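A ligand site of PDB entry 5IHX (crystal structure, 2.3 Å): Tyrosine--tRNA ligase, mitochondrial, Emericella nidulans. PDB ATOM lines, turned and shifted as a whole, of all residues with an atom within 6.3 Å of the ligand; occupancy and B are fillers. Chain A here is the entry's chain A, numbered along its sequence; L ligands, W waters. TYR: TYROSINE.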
ATOM      1  N   TYR A  69     -10.193 -11.264  20.793  1.00  0.00           N
ATOM      2  CA  TYR A  69      -9.287 -11.689  19.727  1.00  0.00           C
ATOM      3  C   TYR A  69      -9.172 -10.680  18.603  1.00  0.00           C
ATOM      4  O   TYR A  69     -10.042  -9.833  18.402  1.00  0.00           O
ATOM      5  CB  TYR A  69      -9.735 -13.044  19.157  1.00  0.00           C
ATOM      6  CG  TYR A  69     -10.676 -12.973  17.976  1.00  0.00           C
ATOM      7  CD1 TYR A  69     -10.182 -13.056  16.669  1.00  0.00           C
ATOM      8  CD2 TYR A  69     -12.050 -12.859  18.146  1.00  0.00           C
ATOM      9  CE1 TYR A  69     -11.035 -13.005  15.578  1.00  0.00           C
ATOM     10  CE2 TYR A  69     -12.907 -12.821  17.054  1.00  0.00           C
ATOM     11  CZ  TYR A  69     -12.393 -12.889  15.782  1.00  0.00           C
ATOM     12  OH  TYR A  69     -13.241 -12.847  14.692  1.00  0.00           O
ATOM     13  N   ALA A  70      -8.048 -10.777  17.893  1.00  0.00           N
ATOM     14  CA  ALA A  70      -7.803  -9.997  16.682  1.00  0.00           C
ATOM     15  C   ALA A  70      -7.307 -10.933  15.608  1.00  0.00           C
ATOM     16  O   ALA A  70      -6.556 -11.864  15.891  1.00  0.00           O
ATOM     17  CB  ALA A  70      -6.802  -8.898  16.946  1.00  0.00           C
ATOM     18  N   GLY A  71      -7.746 -10.709  14.377  1.00  0.00           N
ATOM     19  CA  GLY A  71      -7.372 -11.557  13.255  1.00  0.00           C
ATOM     20  C   GLY A  71      -6.400 -10.881  12.306  1.00  0.00           C
ATOM     21  O   GLY A  71      -6.376  -9.653  12.206  1.00  0.00           O
ATOM     22  N   VAL A  72      -5.594 -11.687  11.625  1.00  0.00           N
ATOM     23  CA  VAL A  72      -4.685 -11.169  10.609  1.00  0.00           C
ATOM     24  C   VAL A  72      -4.552 -12.188   9.487  1.00  0.00           C
ATOM     25  O   VAL A  72      -4.365 -13.385   9.740  1.00  0.00           O
ATOM     26  CB  VAL A  72      -3.286 -10.837  11.201  1.00  0.00           C
ATOM     27  CG1 VAL A  72      -2.690 -12.045  11.924  1.00  0.00           C
ATOM     28  CG2 VAL A  72      -2.339 -10.343  10.112  1.00  0.00           C
ATOM     29  N   ASP A  73      -4.665 -11.714   8.249  1.00  0.00           N
ATOM     30  CA  ASP A  73      -4.518 -12.574   7.081  1.00  0.00           C
ATOM     31  C   ASP A  73      -3.084 -12.493   6.548  1.00  0.00           C
ATOM     32  O   ASP A  73      -2.597 -11.394   6.249  1.00  0.00           O
ATOM     33  CB  ASP A  73      -5.508 -12.186   5.979  1.00  0.00           C
ATOM     34  CG  ASP A  73      -6.912 -12.700   6.242  1.00  0.00           C
ATOM     35  OD1 ASP A  73      -7.823 -12.385   5.444  1.00  0.00           O
ATOM     36  OD2 ASP A  73      -7.108 -13.454   7.226  1.00  0.00           O
ATOM     37  N   HIS A  83      -0.152  -3.096  11.320  1.00  0.00           N
ATOM     38  CA  HIS A  83      -0.957  -4.156  11.931  1.00  0.00           C
ATOM     39  C   HIS A  83      -1.009  -4.083  13.449  1.00  0.00           C
ATOM     40  O   HIS A  83      -1.772  -4.809  14.084  1.00  0.00           O
ATOM     41  CB  HIS A  83      -0.419  -5.545  11.569  1.00  0.00           C
ATOM     42  CG  HIS A  83      -0.619  -5.942  10.138  1.00  0.00           C
ATOM     43  ND1 HIS A  83       0.383  -5.888   9.193  1.00  0.00           N
ATOM     44  CD2 HIS A  83      -1.705  -6.456   9.516  1.00  0.00           C
ATOM     45  CE1 HIS A  83      -0.085  -6.328   8.037  1.00  0.00           C
ATOM     46  NE2 HIS A  83      -1.343  -6.677   8.209  1.00  0.00           N
ATOM     47  N   LEU A 103      -5.616 -14.650  15.977  1.00  0.00           N
ATOM     48  CA  LEU A 103      -6.159 -15.512  14.927  1.00  0.00           C
ATOM     49  C   LEU A 103      -5.449 -15.290  13.609  1.00  0.00           C
ATOM     50  O   LEU A 103      -5.526 -14.210  13.026  1.00  0.00           O
ATOM     51  CB  LEU A 103      -7.662 -15.265  14.759  1.00  0.00           C
ATOM     52  CG  LEU A 103      -8.340 -16.131  13.702  1.00  0.00           C
ATOM     53  CD1 LEU A 103      -8.323 -17.597  14.118  1.00  0.00           C
ATOM     54  CD2 LEU A 103      -9.766 -15.663  13.448  1.00  0.00           C
ATOM     55  N   LEU A 104      -4.771 -16.328  13.127  1.00  0.00           N
ATOM     56  CA  LEU A 104      -4.098 -16.280  11.840  1.00  0.00           C
ATOM     57  C   LEU A 104      -5.056 -16.804  10.774  1.00  0.00           C
ATOM     58  O   LEU A 104      -5.497 -17.950  10.829  1.00  0.00           O
ATOM     59  CB  LEU A 104      -2.804 -17.090  11.869  1.00  0.00           C
ATOM     60  CG  LEU A 104      -1.937 -17.086  10.603  1.00  0.00           C
ATOM     61  CD1 LEU A 104      -1.497 -15.669  10.230  1.00  0.00           C
ATOM     62  CD2 LEU A 104      -0.737 -17.988  10.800  1.00  0.00           C
ATOM     63  N   GLY A 105      -5.383 -15.945   9.814  1.00  0.00           N
ATOM     64  CA  GLY A 105      -6.371 -16.283   8.805  1.00  0.00           C
ATOM     65  C   GLY A 105      -5.805 -17.070   7.646  1.00  0.00           C
ATOM     66  O   GLY A 105      -5.819 -16.597   6.510  1.00  0.00           O
ATOM     67  N   THR A 108      -8.931 -17.862   5.373  1.00  0.00           N
ATOM     68  CA  THR A 108      -9.613 -16.675   4.879  1.00  0.00           C
ATOM     69  C   THR A 108      -8.706 -15.819   4.001  1.00  0.00           C
ATOM     70  O   THR A 108      -9.183 -14.948   3.265  1.00  0.00           O
ATOM     71  CB  THR A 108     -10.133 -15.807   6.043  1.00  0.00           C
ATOM     72  OG1 THR A 108      -9.106 -15.657   7.027  1.00  0.00           O
ATOM     73  CG2 THR A 108     -11.357 -16.454   6.695  1.00  0.00           C
ATOM     74  N   ASP A 113      -9.981 -10.555   2.003  1.00  0.00           N
ATOM     75  CA  ASP A 113     -10.948  -9.587   2.503  1.00  0.00           C
ATOM     76  C   ASP A 113     -11.186  -8.473   1.487  1.00  0.00           C
ATOM     77  O   ASP A 113     -10.259  -7.727   1.170  1.00  0.00           O
ATOM     78  CB  ASP A 113     -10.479  -8.995   3.836  1.00  0.00           C
ATOM     79  CG  ASP A 113     -11.581  -8.278   4.574  1.00  0.00           C
ATOM     80  OD1 ASP A 113     -11.438  -8.066   5.798  1.00  0.00           O
ATOM     81  OD2 ASP A 113     -12.598  -7.926   3.937  1.00  0.00           O
ATOM     82  N   THR A 115     -12.746  -5.707   1.768  1.00  0.00           N
ATOM     83  CA  THR A 115     -12.922  -4.371   2.338  1.00  0.00           C
ATOM     84  C   THR A 115     -11.780  -3.438   1.983  1.00  0.00           C
ATOM     85  O   THR A 115     -10.612  -3.832   1.958  1.00  0.00           O
ATOM     86  CB  THR A 115     -13.051  -4.438   3.876  1.00  0.00           C
ATOM     87  OG1 THR A 115     -11.831  -4.945   4.438  1.00  0.00           O
ATOM     88  CG2 THR A 115     -14.215  -5.328   4.286  1.00  0.00           C
ATOM     89  N   ASN A 169      -7.187 -20.371  11.599  1.00  0.00           N
ATOM     90  CA  ASN A 169      -8.576 -20.733  11.307  1.00  0.00           C
ATOM     91  C   ASN A 169      -8.673 -21.869  10.287  1.00  0.00           C
ATOM     92  O   ASN A 169      -9.763 -22.358   9.999  1.00  0.00           O
ATOM     93  CB  ASN A 169      -9.376 -19.504  10.828  1.00  0.00           C
ATOM     94  CG  ASN A 169      -8.858 -18.901   9.537  1.00  0.00           C
ATOM     95  OD1 ASN A 169      -7.966 -19.453   8.882  1.00  0.00           O
ATOM     96  ND2 ASN A 169      -9.435 -17.769   9.147  1.00  0.00           N
ATOM     97  N   TYR A 217     -16.966 -13.686   2.269  1.00  0.00           N
ATOM     98  CA  TYR A 217     -15.914 -13.455   3.255  1.00  0.00           C
ATOM     99  C   TYR A 217     -16.452 -13.020   4.628  1.00  0.00           C
ATOM    100  O   TYR A 217     -16.003 -13.532   5.649  1.00  0.00           O
ATOM    101  CB  TYR A 217     -14.908 -12.412   2.736  1.00  0.00           C
ATOM    102  CG  TYR A 217     -13.693 -12.259   3.624  1.00  0.00           C
ATOM    103  CD1 TYR A 217     -12.518 -12.938   3.338  1.00  0.00           C
ATOM    104  CD2 TYR A 217     -13.724 -11.425   4.745  1.00  0.00           C
ATOM    105  CE1 TYR A 217     -11.406 -12.805   4.146  1.00  0.00           C
ATOM    106  CE2 TYR A 217     -12.612 -11.291   5.553  1.00  0.00           C
ATOM    107  CZ  TYR A 217     -11.452 -11.981   5.253  1.00  0.00           C
ATOM    108  OH  TYR A 217     -10.346 -11.852   6.050  1.00  0.00           O
ATOM    109  N   MET A 220     -17.447 -15.914   6.671  1.00  0.00           N
ATOM    110  CA  MET A 220     -16.314 -16.681   7.165  1.00  0.00           C
ATOM    111  C   MET A 220     -15.722 -16.037   8.418  1.00  0.00           C
ATOM    112  O   MET A 220     -15.423 -16.725   9.397  1.00  0.00           O
ATOM    113  CB  MET A 220     -15.230 -16.820   6.091  1.00  0.00           C
ATOM    114  CG  MET A 220     -15.649 -17.650   4.891  1.00  0.00           C
ATOM    115  SD  MET A 220     -14.323 -17.829   3.684  1.00  0.00           S
ATOM    116  CE  MET A 220     -13.215 -18.943   4.546  1.00  0.00           C
ATOM    117  N   GLN A 221     -15.566 -14.717   8.391  1.00  0.00           N
ATOM    118  CA  GLN A 221     -15.082 -13.995   9.558  1.00  0.00           C
ATOM    119  C   GLN A 221     -16.052 -14.158  10.729  1.00  0.00           C
ATOM    120  O   GLN A 221     -15.646 -14.297  11.878  1.00  0.00           O
ATOM    121  CB  GLN A 221     -14.873 -12.509   9.238  1.00  0.00           C
ATOM    122  CG  GLN A 221     -14.248 -11.725  10.390  1.00  0.00           C
ATOM    123  CD  GLN A 221     -13.453 -10.510   9.944  1.00  0.00           C
ATOM    124  OE1 GLN A 221     -13.035 -10.417   8.788  1.00  0.00           O
ATOM    125  NE2 GLN A 221     -13.233  -9.586  10.865  1.00  0.00           N
ATOM    126  N   ALA A 222     -17.342 -14.128  10.420  1.00  0.00           N
ATOM    127  CA  ALA A 222     -18.368 -14.309  11.438  1.00  0.00           C
ATOM    128  C   ALA A 222     -18.275 -15.697  12.038  1.00  0.00           C
ATOM    129  O   ALA A 222     -18.383 -15.868  13.259  1.00  0.00           O
ATOM    130  CB  ALA A 222     -19.750 -14.085  10.846  1.00  0.00           C
ATOM    131  N   ASP A 224     -15.596 -17.608  12.106  1.00  0.00           N
ATOM    132  CA  ASP A 224     -14.376 -17.588  12.920  1.00  0.00           C
ATOM    133  C   ASP A 224     -14.690 -17.154  14.339  1.00  0.00           C
ATOM    134  O   ASP A 224     -14.311 -17.815  15.301  1.00  0.00           O
ATOM    135  CB  ASP A 224     -13.325 -16.646  12.333  1.00  0.00           C
ATOM    136  CG  ASP A 224     -12.623 -17.222  11.120  1.00  0.00           C
ATOM    137  OD1 ASP A 224     -11.912 -16.449  10.442  1.00  0.00           O
ATOM    138  OD2 ASP A 224     -12.776 -18.426  10.837  1.00  0.00           O
ATOM    139  N   TRP A 225     -15.390 -16.024  14.455  1.00  0.00           N
ATOM    140  CA  TRP A 225     -15.757 -15.476  15.756  1.00  0.00           C
ATOM    141  C   TRP A 225     -16.597 -16.484  16.531  1.00  0.00           C
ATOM    142  O   TRP A 225     -16.338 -16.743  17.707  1.00  0.00           O
ATOM    143  CB  TRP A 225     -16.525 -14.173  15.586  1.00  0.00           C
ATOM    144  CG  TRP A 225     -16.623 -13.344  16.836  1.00  0.00           C
ATOM    145  CD1 TRP A 225     -16.276 -13.726  18.096  1.00  0.00           C
ATOM    146  CD2 TRP A 225     -17.104 -11.998  16.936  1.00  0.00           C
ATOM    147  NE1 TRP A 225     -16.509 -12.702  18.984  1.00  0.00           N
ATOM    148  CE2 TRP A 225     -17.011 -11.633  18.296  1.00  0.00           C
ATOM    149  CE3 TRP A 225     -17.602 -11.074  16.020  1.00  0.00           C
ATOM    150  CZ2 TRP A 225     -17.405 -10.371  18.753  1.00  0.00           C
ATOM    151  CZ3 TRP A 225     -17.986  -9.829  16.480  1.00  0.00           C
ATOM    152  CH2 TRP A 225     -17.891  -9.487  17.831  1.00  0.00           C
ATOM    153  N   LEU A 228     -14.624 -19.116  18.143  1.00  0.00           N
ATOM    154  CA  LEU A 228     -13.923 -18.629  19.334  1.00  0.00           C
ATOM    155  C   LEU A 228     -14.902 -18.249  20.438  1.00  0.00           C
ATOM    156  O   LEU A 228     -14.620 -18.426  21.625  1.00  0.00           O
ATOM    157  CB  LEU A 228     -13.042 -17.433  18.987  1.00  0.00           C
ATOM    158  CG  LEU A 228     -11.946 -17.686  17.941  1.00  0.00           C
ATOM    159  CD1 LEU A 228     -11.156 -16.412  17.675  1.00  0.00           C
ATOM    160  CD2 LEU A 228     -11.007 -18.815  18.372  1.00  0.00           C
ATOM    161  N   GLN A 236     -14.280  -8.947  19.845  1.00  0.00           N
ATOM    162  CA  GLN A 236     -13.322  -8.870  18.746  1.00  0.00           C
ATOM    163  C   GLN A 236     -12.815  -7.446  18.570  1.00  0.00           C
ATOM    164  O   GLN A 236     -13.598  -6.490  18.647  1.00  0.00           O
ATOM    165  CB  GLN A 236     -13.935  -9.352  17.431  1.00  0.00           C
ATOM    166  CG  GLN A 236     -12.973  -9.231  16.239  1.00  0.00           C
ATOM    167  CD  GLN A 236     -13.548  -9.717  14.921  1.00  0.00           C
ATOM    168  OE1 GLN A 236     -12.885  -9.649  13.887  1.00  0.00           O
ATOM    169  NE2 GLN A 236     -14.772 -10.229  14.945  1.00  0.00           N
ATOM    170  N   GLY A 239      -8.723  -3.447  12.974  1.00  0.00           N
ATOM    171  CA  GLY A 239      -8.369  -2.143  12.456  1.00  0.00           C
ATOM    172  C   GLY A 239      -9.609  -1.323  12.152  1.00  0.00           C
ATOM    173  O   GLY A 239     -10.722  -1.839  12.147  1.00  0.00           O
ATOM    174  N   ASP A 241     -10.833  -0.147   9.447  1.00  0.00           N
ATOM    175  CA  ASP A 241     -11.595  -0.550   8.272  1.00  0.00           C
ATOM    176  C   ASP A 241     -12.385  -1.844   8.477  1.00  0.00           C
ATOM    177  O   ASP A 241     -13.060  -2.322   7.568  1.00  0.00           O
ATOM    178  CB  ASP A 241     -10.666  -0.721   7.066  1.00  0.00           C
ATOM    179  CG  ASP A 241      -9.729  -1.904   7.214  1.00  0.00           C
ATOM    180  OD1 ASP A 241      -9.343  -2.215   8.356  1.00  0.00           O
ATOM    181  OD2 ASP A 241      -9.386  -2.515   6.186  1.00  0.00           O
ATOM    182  N   GLN A 242     -12.299  -2.406   9.683  1.00  0.00           N
ATOM    183  CA  GLN A 242     -12.972  -3.670   9.982  1.00  0.00           C
ATOM    184  C   GLN A 242     -14.318  -3.477  10.664  1.00  0.00           C
ATOM    185  O   GLN A 242     -14.932  -4.452  11.096  1.00  0.00           O
ATOM    186  CB  GLN A 242     -12.064  -4.547  10.845  1.00  0.00           C
ATOM    187  CG  GLN A 242     -10.851  -5.091  10.111  1.00  0.00           C
ATOM    188  CD  GLN A 242     -11.231  -6.015   8.984  1.00  0.00           C
ATOM    189  OE1 GLN A 242     -11.950  -6.999   9.190  1.00  0.00           O
ATOM    190  NE2 GLN A 242     -10.792  -5.692   7.771  1.00  0.00           N
ATOM    191  N   ASN A 245     -17.144  -5.579   8.938  1.00  0.00           N
ATOM    192  CA  ASN A 245     -17.047  -7.014   9.205  1.00  0.00           C
ATOM    193  C   ASN A 245     -17.393  -7.369  10.642  1.00  0.00           C
ATOM    194  O   ASN A 245     -18.053  -8.371  10.901  1.00  0.00           O
ATOM    195  CB  ASN A 245     -15.650  -7.539   8.874  1.00  0.00           C
ATOM    196  CG  ASN A 245     -15.347  -7.510   7.382  1.00  0.00           C
ATOM    197  OD1 ASN A 245     -16.256  -7.587   6.550  1.00  0.00           O
ATOM    198  ND2 ASN A 245     -14.071  -7.429   7.030  1.00  0.00           N
HETATM  199  N   TYR L   1     -10.387  -9.719   7.826  1.00  0.00           N
HETATM  200  CA  TYR L   1      -9.275  -9.172   8.656  1.00  0.00           C
HETATM  201  C   TYR L   1      -8.323  -8.344   7.809  1.00  0.00           C
HETATM  202  O   TYR L   1      -7.660  -7.421   8.309  1.00  0.00           O
HETATM  203  CB  TYR L   1      -8.515 -10.311   9.348  1.00  0.00           C
HETATM  204  CG  TYR L   1      -9.408 -11.288  10.060  1.00  0.00           C
HETATM  205  CD1 TYR L   1     -10.152 -10.898  11.170  1.00  0.00           C
HETATM  206  CD2 TYR L   1      -9.524 -12.598   9.626  1.00  0.00           C
HETATM  207  CE1 TYR L   1     -10.976 -11.791  11.821  1.00  0.00           C
HETATM  208  CE2 TYR L   1     -10.343 -13.499  10.278  1.00  0.00           C
HETATM  209  CZ  TYR L   1     -11.061 -13.087  11.372  1.00  0.00           C
HETATM  210  OH  TYR L   1     -11.885 -13.980  12.022  1.00  0.00           O
HETATM  211  OXT TYR L   1      -8.183  -8.574   6.612  1.00  0.00           O
HETATM  212  O   HOH W   1      -4.984  -8.779   7.974  1.00  0.00           O
HETATM  213  O   HOH W   2      -8.881  -7.870  11.811  1.00  0.00           O
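Gly 71 touches the ligand.
N of Val 72 touches CB of the ligand (3.95 Å).
Asp 73 touches the ligand (OD2 to CD2, 3.5 Å).
Leu 103 touches the ligand.
Gln 236 touches the ligand.
Hydrophobic or aromatic side chains within 4 Å of the ligand: Tyr 69, Leu 103 and Tyr 217.
The nearest printed residue that does not touch the ligand is Thr 108 (4.04 Å).
The side-chain hydroxyl (OH) of Tyr 217 is in hydrogen-bond range of a nitrogen (N) of the ligand (2.8 Å).
N of the ligand is in salt-bridge range of OD1 of Asp 113 (2.8 Å).
OE1 of Gln 221 sits at hydrogen-bond distance from N of the ligand, 2.9 Å away.
The side-chain carboxylate (OD1) of Asp 224 sits at hydrogen-bond distance from an oxygen (OH) of the ligand (2.9 Å).
The side-chain hydroxyl of Tyr 69 sits at hydrogen-bond distance from an oxygen (OH) of the ligand (3.2 Å).
The side-chain amide oxygen (OE1) of Gln 242 lies within hydrogen-bond range of a nitrogen (N) of the ligand (3.4 Å).
OH of Tyr 217 sits at hydrogen-bond distance from OD1 of Asp 73 (2.6 Å).
The side-chain carboxylate (OD1) of Asp 113 lies within hydrogen-bond range of the side-chain amide nitrogen (NE2) of Gln 242 (3.2 Å).
NE2 of Gln 221 lies within hydrogen-bond range of OE1 of Gln 242, 3.3 Å away.
The side-chain amide nitrogen of Gln 221 sits at hydrogen-bond distance from the side-chain amide oxygen of Gln 236 (3.0 Å).
OD1 of Asp 224 is in hydrogen-bond range of ND2 of Asn 169 (3.1 Å).
The side-chain amide nitrogen (NE2) of Gln 236 lies within hydrogen-bond range of the side-chain hydroxyl (OH) of Tyr 69 (3.0 Å).
The side-chain amide oxygen (OE1) of Gln 242 lies within hydrogen-bond range of the side-chain amide nitrogen (ND2) of Asn 245 (3.1 Å).
O of Val 72 lies within hydrogen-bond range of N of Gly 105 (2.8 Å).
Water W1 lies within hydrogen-bond range of N of Asp 73 and O of the ligand.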
